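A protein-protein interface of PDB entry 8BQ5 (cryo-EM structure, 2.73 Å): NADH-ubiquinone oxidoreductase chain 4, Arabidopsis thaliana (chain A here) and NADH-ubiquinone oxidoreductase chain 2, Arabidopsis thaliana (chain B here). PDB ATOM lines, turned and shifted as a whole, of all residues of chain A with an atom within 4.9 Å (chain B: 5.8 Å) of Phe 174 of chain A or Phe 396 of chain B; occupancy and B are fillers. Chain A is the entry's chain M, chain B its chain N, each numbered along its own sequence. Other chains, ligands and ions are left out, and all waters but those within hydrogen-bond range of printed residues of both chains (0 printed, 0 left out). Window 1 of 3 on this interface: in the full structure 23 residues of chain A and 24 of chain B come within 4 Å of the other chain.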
ATOM      1  N   LEU A 150      -5.719  10.716  22.792  1.00  0.00           N
ATOM      2  CA  LEU A 150      -6.106  12.067  22.303  1.00  0.00           C
ATOM      3  C   LEU A 150      -5.513  12.375  20.922  1.00  0.00           C
ATOM      4  O   LEU A 150      -6.216  13.033  20.153  1.00  0.00           O
ATOM      5  CB  LEU A 150      -5.646  13.102  23.339  1.00  0.00           C
ATOM      6  CG  LEU A 150      -6.614  13.406  24.481  1.00  0.00           C
ATOM      7  CD1 LEU A 150      -7.003  12.146  25.239  1.00  0.00           C
ATOM      8  CD2 LEU A 150      -6.017  14.427  25.436  1.00  0.00           C
ATOM      9  N   ILE A 151      -4.285  11.935  20.617  1.00  0.00           N
ATOM     10  CA  ILE A 151      -3.619  12.277  19.361  1.00  0.00           C
ATOM     11  C   ILE A 151      -4.338  11.645  18.168  1.00  0.00           C
ATOM     12  O   ILE A 151      -4.716  12.376  17.234  1.00  0.00           O
ATOM     13  CB  ILE A 151      -2.132  11.882  19.399  1.00  0.00           C
ATOM     14  CG1 ILE A 151      -1.360  12.795  20.351  1.00  0.00           C
ATOM     15  CG2 ILE A 151      -1.529  11.924  18.007  1.00  0.00           C
ATOM     16  CD1 ILE A 151       0.003  12.269  20.719  1.00  0.00           C
ATOM     17  N   PHE A 154      -7.820  13.250  17.792  1.00  0.00           N
ATOM     18  CA  PHE A 154      -7.643  14.588  17.245  1.00  0.00           C
ATOM     19  C   PHE A 154      -7.457  14.530  15.737  1.00  0.00           C
ATOM     20  O   PHE A 154      -8.110  15.265  14.985  1.00  0.00           O
ATOM     21  CB  PHE A 154      -6.432  15.234  17.929  1.00  0.00           C
ATOM     22  CG  PHE A 154      -6.220  16.684  17.600  1.00  0.00           C
ATOM     23  CD1 PHE A 154      -7.146  17.641  17.971  1.00  0.00           C
ATOM     24  CD2 PHE A 154      -5.063  17.094  16.957  1.00  0.00           C
ATOM     25  CE1 PHE A 154      -6.935  18.974  17.684  1.00  0.00           C
ATOM     26  CE2 PHE A 154      -4.847  18.425  16.668  1.00  0.00           C
ATOM     27  CZ  PHE A 154      -5.783  19.367  17.031  1.00  0.00           C
ATOM     28  N   ALA A 170     -12.424  19.724  17.400  1.00  0.00           N
ATOM     29  CA  ALA A 170     -11.220  19.011  17.807  1.00  0.00           C
ATOM     30  C   ALA A 170     -10.462  19.773  18.887  1.00  0.00           C
ATOM     31  O   ALA A 170      -9.940  19.166  19.833  1.00  0.00           O
ATOM     32  CB  ALA A 170     -10.329  18.757  16.592  1.00  0.00           C
ATOM     33  N   TYR A 171     -10.391  21.104  18.765  1.00  0.00           N
ATOM     34  CA  TYR A 171      -9.752  21.910  19.802  1.00  0.00           C
ATOM     35  C   TYR A 171     -10.416  21.691  21.157  1.00  0.00           C
ATOM     36  O   TYR A 171      -9.744  21.408  22.158  1.00  0.00           O
ATOM     37  CB  TYR A 171      -9.811  23.389  19.424  1.00  0.00           C
ATOM     38  CG  TYR A 171      -8.713  23.847  18.498  1.00  0.00           C
ATOM     39  CD1 TYR A 171      -7.478  23.218  18.483  1.00  0.00           C
ATOM     40  CD2 TYR A 171      -8.917  24.915  17.638  1.00  0.00           C
ATOM     41  CE1 TYR A 171      -6.478  23.641  17.636  1.00  0.00           C
ATOM     42  CE2 TYR A 171      -7.927  25.342  16.791  1.00  0.00           C
ATOM     43  CZ  TYR A 171      -6.709  24.706  16.791  1.00  0.00           C
ATOM     44  OH  TYR A 171      -5.719  25.139  15.942  1.00  0.00           O
ATOM     45  N   GLN A 172     -11.745  21.825  21.201  1.00  0.00           N
ATOM     46  CA  GLN A 172     -12.462  21.661  22.462  1.00  0.00           C
ATOM     47  C   GLN A 172     -12.284  20.257  23.026  1.00  0.00           C
ATOM     48  O   GLN A 172     -12.063  20.094  24.232  1.00  0.00           O
ATOM     49  CB  GLN A 172     -13.941  21.984  22.269  1.00  0.00           C
ATOM     50  CG  GLN A 172     -14.326  23.378  22.713  1.00  0.00           C
ATOM     51  CD  GLN A 172     -15.637  23.835  22.117  1.00  0.00           C
ATOM     52  OE1 GLN A 172     -15.675  24.787  21.340  1.00  0.00           O
ATOM     53  NE2 GLN A 172     -16.716  23.147  22.461  1.00  0.00           N
ATOM     54  N   PHE A 173     -12.368  19.234  22.169  1.00  0.00           N
ATOM     55  CA  PHE A 173     -12.173  17.860  22.623  1.00  0.00           C
ATOM     56  C   PHE A 173     -10.816  17.689  23.295  1.00  0.00           C
ATOM     57  O   PHE A 173     -10.724  17.249  24.455  1.00  0.00           O
ATOM     58  CB  PHE A 173     -12.310  16.910  21.431  1.00  0.00           C
ATOM     59  CG  PHE A 173     -11.805  15.520  21.690  1.00  0.00           C
ATOM     60  CD1 PHE A 173     -12.563  14.615  22.410  1.00  0.00           C
ATOM     61  CD2 PHE A 173     -10.571  15.113  21.202  1.00  0.00           C
ATOM     62  CE1 PHE A 173     -12.103  13.335  22.644  1.00  0.00           C
ATOM     63  CE2 PHE A 173     -10.104  13.834  21.435  1.00  0.00           C
ATOM     64  CZ  PHE A 173     -10.871  12.944  22.158  1.00  0.00           C
ATOM     65  N   PHE A 174      -9.748  18.075  22.587  1.00  0.00           N
ATOM     66  CA  PHE A 174      -8.401  17.883  23.108  1.00  0.00           C
ATOM     67  C   PHE A 174      -8.209  18.639  24.415  1.00  0.00           C
ATOM     68  O   PHE A 174      -7.650  18.101  25.378  1.00  0.00           O
ATOM     69  CB  PHE A 174      -7.369  18.324  22.066  1.00  0.00           C
ATOM     70  CG  PHE A 174      -6.071  17.562  22.130  1.00  0.00           C
ATOM     71  CD1 PHE A 174      -5.272  17.615  23.258  1.00  0.00           C
ATOM     72  CD2 PHE A 174      -5.655  16.787  21.063  1.00  0.00           C
ATOM     73  CE1 PHE A 174      -4.082  16.916  23.319  1.00  0.00           C
ATOM     74  CE2 PHE A 174      -4.466  16.086  21.117  1.00  0.00           C
ATOM     75  CZ  PHE A 174      -3.679  16.150  22.247  1.00  0.00           C
ATOM     76  N   LEU A 175      -8.701  19.878  24.484  1.00  0.00           N
ATOM     77  CA  LEU A 175      -8.408  20.704  25.651  1.00  0.00           C
ATOM     78  C   LEU A 175      -9.192  20.251  26.881  1.00  0.00           C
ATOM     79  O   LEU A 175      -8.633  20.173  27.986  1.00  0.00           O
ATOM     80  CB  LEU A 175      -8.681  22.170  25.324  1.00  0.00           C
ATOM     81  CG  LEU A 175      -7.592  22.790  24.440  1.00  0.00           C
ATOM     82  CD1 LEU A 175      -8.032  24.124  23.859  1.00  0.00           C
ATOM     83  CD2 LEU A 175      -6.289  22.937  25.198  1.00  0.00           C
ATOM     84  N   TYR A 176     -10.483  19.942  26.719  1.00  0.00           N
ATOM     85  CA  TYR A 176     -11.265  19.431  27.842  1.00  0.00           C
ATOM     86  C   TYR A 176     -10.653  18.147  28.389  1.00  0.00           C
ATOM     87  O   TYR A 176     -10.431  18.003  29.607  1.00  0.00           O
ATOM     88  CB  TYR A 176     -12.706  19.183  27.396  1.00  0.00           C
ATOM     89  CG  TYR A 176     -13.653  20.325  27.656  1.00  0.00           C
ATOM     90  CD1 TYR A 176     -14.309  20.443  28.872  1.00  0.00           C
ATOM     91  CD2 TYR A 176     -13.900  21.280  26.680  1.00  0.00           C
ATOM     92  CE1 TYR A 176     -15.180  21.481  29.112  1.00  0.00           C
ATOM     93  CE2 TYR A 176     -14.770  22.322  26.911  1.00  0.00           C
ATOM     94  CZ  TYR A 176     -15.407  22.418  28.129  1.00  0.00           C
ATOM     95  OH  TYR A 176     -16.274  23.455  28.367  1.00  0.00           O
ATOM     96  N   THR A 177     -10.352  17.204  27.491  1.00  0.00           N
ATOM     97  CA  THR A 177      -9.816  15.928  27.939  1.00  0.00           C
ATOM     98  C   THR A 177      -8.451  16.098  28.597  1.00  0.00           C
ATOM     99  O   THR A 177      -8.143  15.419  29.584  1.00  0.00           O
ATOM    100  CB  THR A 177      -9.750  14.965  26.761  1.00  0.00           C
ATOM    101  OG1 THR A 177     -10.945  15.095  25.981  1.00  0.00           O
ATOM    102  CG2 THR A 177      -9.667  13.577  27.257  1.00  0.00           C
ATOM    103  N   LEU A 178      -7.622  17.010  28.076  1.00  0.00           N
ATOM    104  CA  LEU A 178      -6.313  17.235  28.680  1.00  0.00           C
ATOM    105  C   LEU A 178      -6.436  17.813  30.086  1.00  0.00           C
ATOM    106  O   LEU A 178      -5.709  17.395  30.993  1.00  0.00           O
ATOM    107  CB  LEU A 178      -5.476  18.158  27.798  1.00  0.00           C
ATOM    108  CG  LEU A 178      -4.104  18.482  28.390  1.00  0.00           C
ATOM    109  CD1 LEU A 178      -3.200  17.271  28.310  1.00  0.00           C
ATOM    110  CD2 LEU A 178      -3.476  19.672  27.706  1.00  0.00           C
ATOM    111  N   PHE B 391       7.013  16.262  12.356  1.00  0.00           N
ATOM    112  CA  PHE B 391       6.856  17.579  13.025  1.00  0.00           C
ATOM    113  C   PHE B 391       5.752  17.476  14.082  1.00  0.00           C
ATOM    114  O   PHE B 391       5.884  18.112  15.127  1.00  0.00           O
ATOM    115  CB  PHE B 391       6.577  18.664  11.982  1.00  0.00           C
ATOM    116  CG  PHE B 391       6.877  20.080  12.402  1.00  0.00           C
ATOM    117  CD1 PHE B 391       7.707  20.351  13.478  1.00  0.00           C
ATOM    118  CD2 PHE B 391       6.349  21.151  11.700  1.00  0.00           C
ATOM    119  CE1 PHE B 391       7.991  21.656  13.847  1.00  0.00           C
ATOM    120  CE2 PHE B 391       6.631  22.455  12.071  1.00  0.00           C
ATOM    121  CZ  PHE B 391       7.450  22.707  13.146  1.00  0.00           C
ATOM    122  N   SER B 392       4.695  16.710  13.805  1.00  0.00           N
ATOM    123  CA  SER B 392       3.589  16.507  14.776  1.00  0.00           C
ATOM    124  C   SER B 392       4.081  15.718  15.993  1.00  0.00           C
ATOM    125  O   SER B 392       3.679  16.073  17.105  1.00  0.00           O
ATOM    126  CB  SER B 392       2.429  15.814  14.120  1.00  0.00           C
ATOM    127  OG  SER B 392       1.864  16.627  13.106  1.00  0.00           O
ATOM    128  N   ILE B 393       4.904  14.685  15.784  1.00  0.00           N
ATOM    129  CA  ILE B 393       5.478  13.911  16.920  1.00  0.00           C
ATOM    130  C   ILE B 393       6.263  14.889  17.797  1.00  0.00           C
ATOM    131  O   ILE B 393       6.073  14.865  19.026  1.00  0.00           O
ATOM    132  CB  ILE B 393       6.363  12.761  16.405  1.00  0.00           C
ATOM    133  CG1 ILE B 393       5.536  11.656  15.743  1.00  0.00           C
ATOM    134  CG2 ILE B 393       7.243  12.216  17.515  1.00  0.00           C
ATOM    135  CD1 ILE B 393       6.368  10.640  14.997  1.00  0.00           C
ATOM    136  N   THR B 394       7.074  15.747  17.178  1.00  0.00           N
ATOM    137  CA  THR B 394       7.852  16.755  17.931  1.00  0.00           C
ATOM    138  C   THR B 394       6.906  17.700  18.681  1.00  0.00           C
ATOM    139  O   THR B 394       7.174  17.969  19.854  1.00  0.00           O
ATOM    140  CB  THR B 394       8.794  17.516  16.990  1.00  0.00           C
ATOM    141  OG1 THR B 394       9.400  16.558  16.123  1.00  0.00           O
ATOM    142  CG2 THR B 394       9.851  18.312  17.722  1.00  0.00           C
ATOM    143  N   MET B 395       5.850  18.181  18.028  1.00  0.00           N
ATOM    144  CA  MET B 395       4.916  19.152  18.663  1.00  0.00           C
ATOM    145  C   MET B 395       4.165  18.495  19.827  1.00  0.00           C
ATOM    146  O   MET B 395       3.938  19.181  20.834  1.00  0.00           O
ATOM    147  CB  MET B 395       3.894  19.673  17.650  1.00  0.00           C
ATOM    148  CG  MET B 395       4.474  20.597  16.603  1.00  0.00           C
ATOM    149  SD  MET B 395       4.928  22.204  17.288  1.00  0.00           S
ATOM    150  CE  MET B 395       6.715  22.076  17.276  1.00  0.00           C
ATOM    151  N   PHE B 396       3.763  17.233  19.681  1.00  0.00           N
ATOM    152  CA  PHE B 396       3.111  16.559  20.798  1.00  0.00           C
ATOM    153  C   PHE B 396       4.098  16.264  21.918  1.00  0.00           C
ATOM    154  O   PHE B 396       3.722  16.298  23.096  1.00  0.00           O
ATOM    155  CB  PHE B 396       2.427  15.276  20.324  1.00  0.00           C
ATOM    156  CG  PHE B 396       1.165  15.510  19.540  1.00  0.00           C
ATOM    157  CD1 PHE B 396       0.130  16.258  20.073  1.00  0.00           C
ATOM    158  CD2 PHE B 396       1.011  14.971  18.275  1.00  0.00           C
ATOM    159  CE1 PHE B 396      -1.030  16.471  19.354  1.00  0.00           C
ATOM    160  CE2 PHE B 396      -0.146  15.182  17.551  1.00  0.00           C
ATOM    161  CZ  PHE B 396      -1.168  15.933  18.092  1.00  0.00           C
ATOM    162  N   SER B 397       5.359  15.982  21.580  1.00  0.00           N
ATOM    163  CA  SER B 397       6.388  15.881  22.610  1.00  0.00           C
ATOM    164  C   SER B 397       6.568  17.208  23.336  1.00  0.00           C
ATOM    165  O   SER B 397       6.703  17.240  24.564  1.00  0.00           O
ATOM    166  CB  SER B 397       7.707  15.426  21.990  1.00  0.00           C
ATOM    167  OG  SER B 397       8.606  14.972  22.985  1.00  0.00           O
ATOM    168  N   TYR B 398       6.572  18.314  22.589  1.00  0.00           N
ATOM    169  CA  TYR B 398       6.656  19.636  23.204  1.00  0.00           C
ATOM    170  C   TYR B 398       5.498  19.870  24.164  1.00  0.00           C
ATOM    171  O   TYR B 398       5.689  20.401  25.264  1.00  0.00           O
ATOM    172  CB  TYR B 398       6.664  20.716  22.122  1.00  0.00           C
ATOM    173  CG  TYR B 398       8.032  21.192  21.698  1.00  0.00           C
ATOM    174  CD1 TYR B 398       8.886  21.805  22.601  1.00  0.00           C
ATOM    175  CD2 TYR B 398       8.463  21.041  20.388  1.00  0.00           C
ATOM    176  CE1 TYR B 398      10.135  22.244  22.216  1.00  0.00           C
ATOM    177  CE2 TYR B 398       9.709  21.480  19.993  1.00  0.00           C
ATOM    178  CZ  TYR B 398      10.541  22.081  20.910  1.00  0.00           C
ATOM    179  OH  TYR B 398      11.783  22.519  20.522  1.00  0.00           O
ATOM    180  N   ALA B 399       4.286  19.480  23.762  1.00  0.00           N
ATOM    181  CA  ALA B 399       3.115  19.668  24.608  1.00  0.00           C
ATOM    182  C   ALA B 399       3.137  18.776  25.841  1.00  0.00           C
ATOM    183  O   ALA B 399       2.354  19.004  26.768  1.00  0.00           O
ATOM    184  CB  ALA B 399       1.841  19.413  23.803  1.00  0.00           C
ATOM    185  N   GLY B 400       4.009  17.771  25.871  1.00  0.00           N
ATOM    186  CA  GLY B 400       4.128  16.906  27.025  1.00  0.00           C
ATOM    187  C   GLY B 400       3.219  15.700  27.034  1.00  0.00           C
ATOM    188  O   GLY B 400       3.161  14.995  28.044  1.00  0.00           O
ATOM    189  N   ILE B 401       2.508  15.434  25.943  1.00  0.00           N
ATOM    190  CA  ILE B 401       1.586  14.302  25.872  1.00  0.00           C
ATOM    191  C   ILE B 401       2.369  12.998  25.968  1.00  0.00           C
ATOM    192  O   ILE B 401       3.344  12.808  25.228  1.00  0.00           O
ATOM    193  CB  ILE B 401       0.752  14.347  24.581  1.00  0.00           C
ATOM    194  CG1 ILE B 401       0.061  15.704  24.432  1.00  0.00           C
ATOM    195  CG2 ILE B 401      -0.263  13.214  24.557  1.00  0.00           C
ATOM    196  CD1 ILE B 401      -0.823  16.079  25.598  1.00  0.00           C
ATOM    197  N   LEU B 404       5.357  10.238  24.880  1.00  0.00           N
ATOM    198  CA  LEU B 404       6.484  10.892  24.235  1.00  0.00           C
ATOM    199  C   LEU B 404       7.477  11.408  25.273  1.00  0.00           C
ATOM    200  O   LEU B 404       7.154  11.590  26.449  1.00  0.00           O
ATOM    201  CB  LEU B 404       5.994  12.031  23.348  1.00  0.00           C
ATOM    202  CG  LEU B 404       4.992  11.555  22.296  1.00  0.00           C
ATOM    203  CD1 LEU B 404       4.504  12.712  21.457  1.00  0.00           C
ATOM    204  CD2 LEU B 404       5.598  10.470  21.425  1.00  0.00           C
ATOM    205  N   CYS B 437      -0.384  23.170  25.121  1.00  0.00           N
ATOM    206  CA  CYS B 437      -0.988  22.163  24.263  1.00  0.00           C
ATOM    207  C   CYS B 437      -1.795  22.813  23.150  1.00  0.00           C
ATOM    208  O   CYS B 437      -1.726  22.382  21.994  1.00  0.00           O
ATOM    209  CB  CYS B 437      -1.870  21.231  25.088  1.00  0.00           C
ATOM    210  SG  CYS B 437      -2.696  19.946  24.133  1.00  0.00           S
ATOM    211  N   TYR B 440       0.596  24.379  20.548  1.00  0.00           N
ATOM    212  CA  TYR B 440       1.358  23.367  19.825  1.00  0.00           C
ATOM    213  C   TYR B 440       0.480  22.618  18.833  1.00  0.00           C
ATOM    214  O   TYR B 440       0.882  22.409  17.684  1.00  0.00           O
ATOM    215  CB  TYR B 440       2.000  22.380  20.799  1.00  0.00           C
ATOM    216  CG  TYR B 440       3.211  22.919  21.516  1.00  0.00           C
ATOM    217  CD1 TYR B 440       4.261  23.500  20.816  1.00  0.00           C
ATOM    218  CD2 TYR B 440       3.306  22.846  22.896  1.00  0.00           C
ATOM    219  CE1 TYR B 440       5.367  23.993  21.478  1.00  0.00           C
ATOM    220  CE2 TYR B 440       4.398  23.340  23.563  1.00  0.00           C
ATOM    221  CZ  TYR B 440       5.427  23.908  22.853  1.00  0.00           C
ATOM    222  OH  TYR B 440       6.515  24.393  23.533  1.00  0.00           O
ATOM    223  N   ILE B 441      -0.723  22.207  19.250  1.00  0.00           N
ATOM    224  CA  ILE B 441      -1.608  21.490  18.335  1.00  0.00           C
ATOM    225  C   ILE B 441      -2.192  22.397  17.268  1.00  0.00           C
ATOM    226  O   ILE B 441      -2.740  21.895  16.279  1.00  0.00           O
ATOM    227  CB  ILE B 441      -2.751  20.773  19.081  1.00  0.00           C
ATOM    228  CG1 ILE B 441      -3.729  21.779  19.688  1.00  0.00           C
ATOM    229  CG2 ILE B 441      -2.197  19.839  20.145  1.00  0.00           C
ATOM    230  CD1 ILE B 441      -4.982  21.138  20.228  1.00  0.00           C
ATOM    231  N   VAL B 444      -0.296  21.337  14.285  1.00  0.00           N
ATOM    232  CA  VAL B 444      -0.812  20.099  13.707  1.00  0.00           C
ATOM    233  C   VAL B 444      -2.088  20.376  12.926  1.00  0.00           C
ATOM    234  O   VAL B 444      -2.297  19.834  11.835  1.00  0.00           O
ATOM    235  CB  VAL B 444      -1.040  19.045  14.804  1.00  0.00           C
ATOM    236  CG1 VAL B 444      -1.534  17.746  14.188  1.00  0.00           C
ATOM    237  CG2 VAL B 444       0.236  18.819  15.591  1.00  0.00           C
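O of Phe 396 of chain B lies within hydrogen-bond range of N of Ile 401 of chain B (3.2 Å).
Of the 16 printed residues of chain B, 4 touch a printed residue of chain A. Hydrophobic or aromatic side chains of chain B that line the printed part of chain A: Phe 396, Ile 401 and Ile 441. Of the 12 printed residues of chain A, 5 touch a printed residue of chain B. Hydrophobic or aromatic side chains of chain A that line the printed part of chain B: Ile 151, Phe 154, Tyr 171, Phe 174 and Leu 178. Along chain A the printed residues that touch a printed residue of chain B span positions 151 to 178. Among the printed residues, 8 pairs touch across the chains. Among the printed residues, no Asp or Glu carboxylate lies within 4 Å of a Lys or Arg side-chain nitrogen of the other chain.
Among the printed residues, merely in contact across the chains: Ile 151 of chain A with Phe 396 of chain B (3.6 Å), Ile 151 of chain A with Ile 401 of chain B (3.96 Å), Phe 154 of chain A with Ile 441 of chain B (3.7 Å), Tyr 171 of chain A with Ile 441 of chain B (3.7 Å), Phe 174 of chain A with Phe 396 of chain B (3.9 Å), Phe 174 of chain A with Cys 437 of chain B (3.4 Å), Leu 178 of chain A with Ile 401 of chain B (3.8 Å) and Leu 178 of chain A with Cys 437 of chain B (3.4 Å).
Of the printed residues of chain B, Ile 151 of chain A touches Phe 396 and Ile 401. Of the printed residues of chain B, Phe 154 of chain A touches Ile 441. Of chain B, only Phe 396 (3.9 Å) and Cys 437 (3.4 Å) come within 4 Å of Phe 174 of chain A. Of the printed residues of chain B, Leu 178 of chain A touches Ile 401 and Cys 437. Met 395 of chain B touches none of the printed residues of chain A. Of chain A, only Ile 151 (3.6 Å) and Phe 174 (3.9 Å) come within 4 Å of Phe 396 of chain B. Ala 399 of chain B touches none of the printed residues of chain A. Of the printed residues of chain A, Cys 437 of chain B touches Phe 174 and Leu 178. Of the printed residues of chain A, Ile 441 of chain B touches Phe 154 and Tyr 171. The nearest residue of chain B that does not touch Phe 174 of chain A is Ile 401 of chain B (4.1 Å). The nearest printed residue of chain B that does not touch Tyr 171 of chain A is Cys 437 of chain B (6.6 Å).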
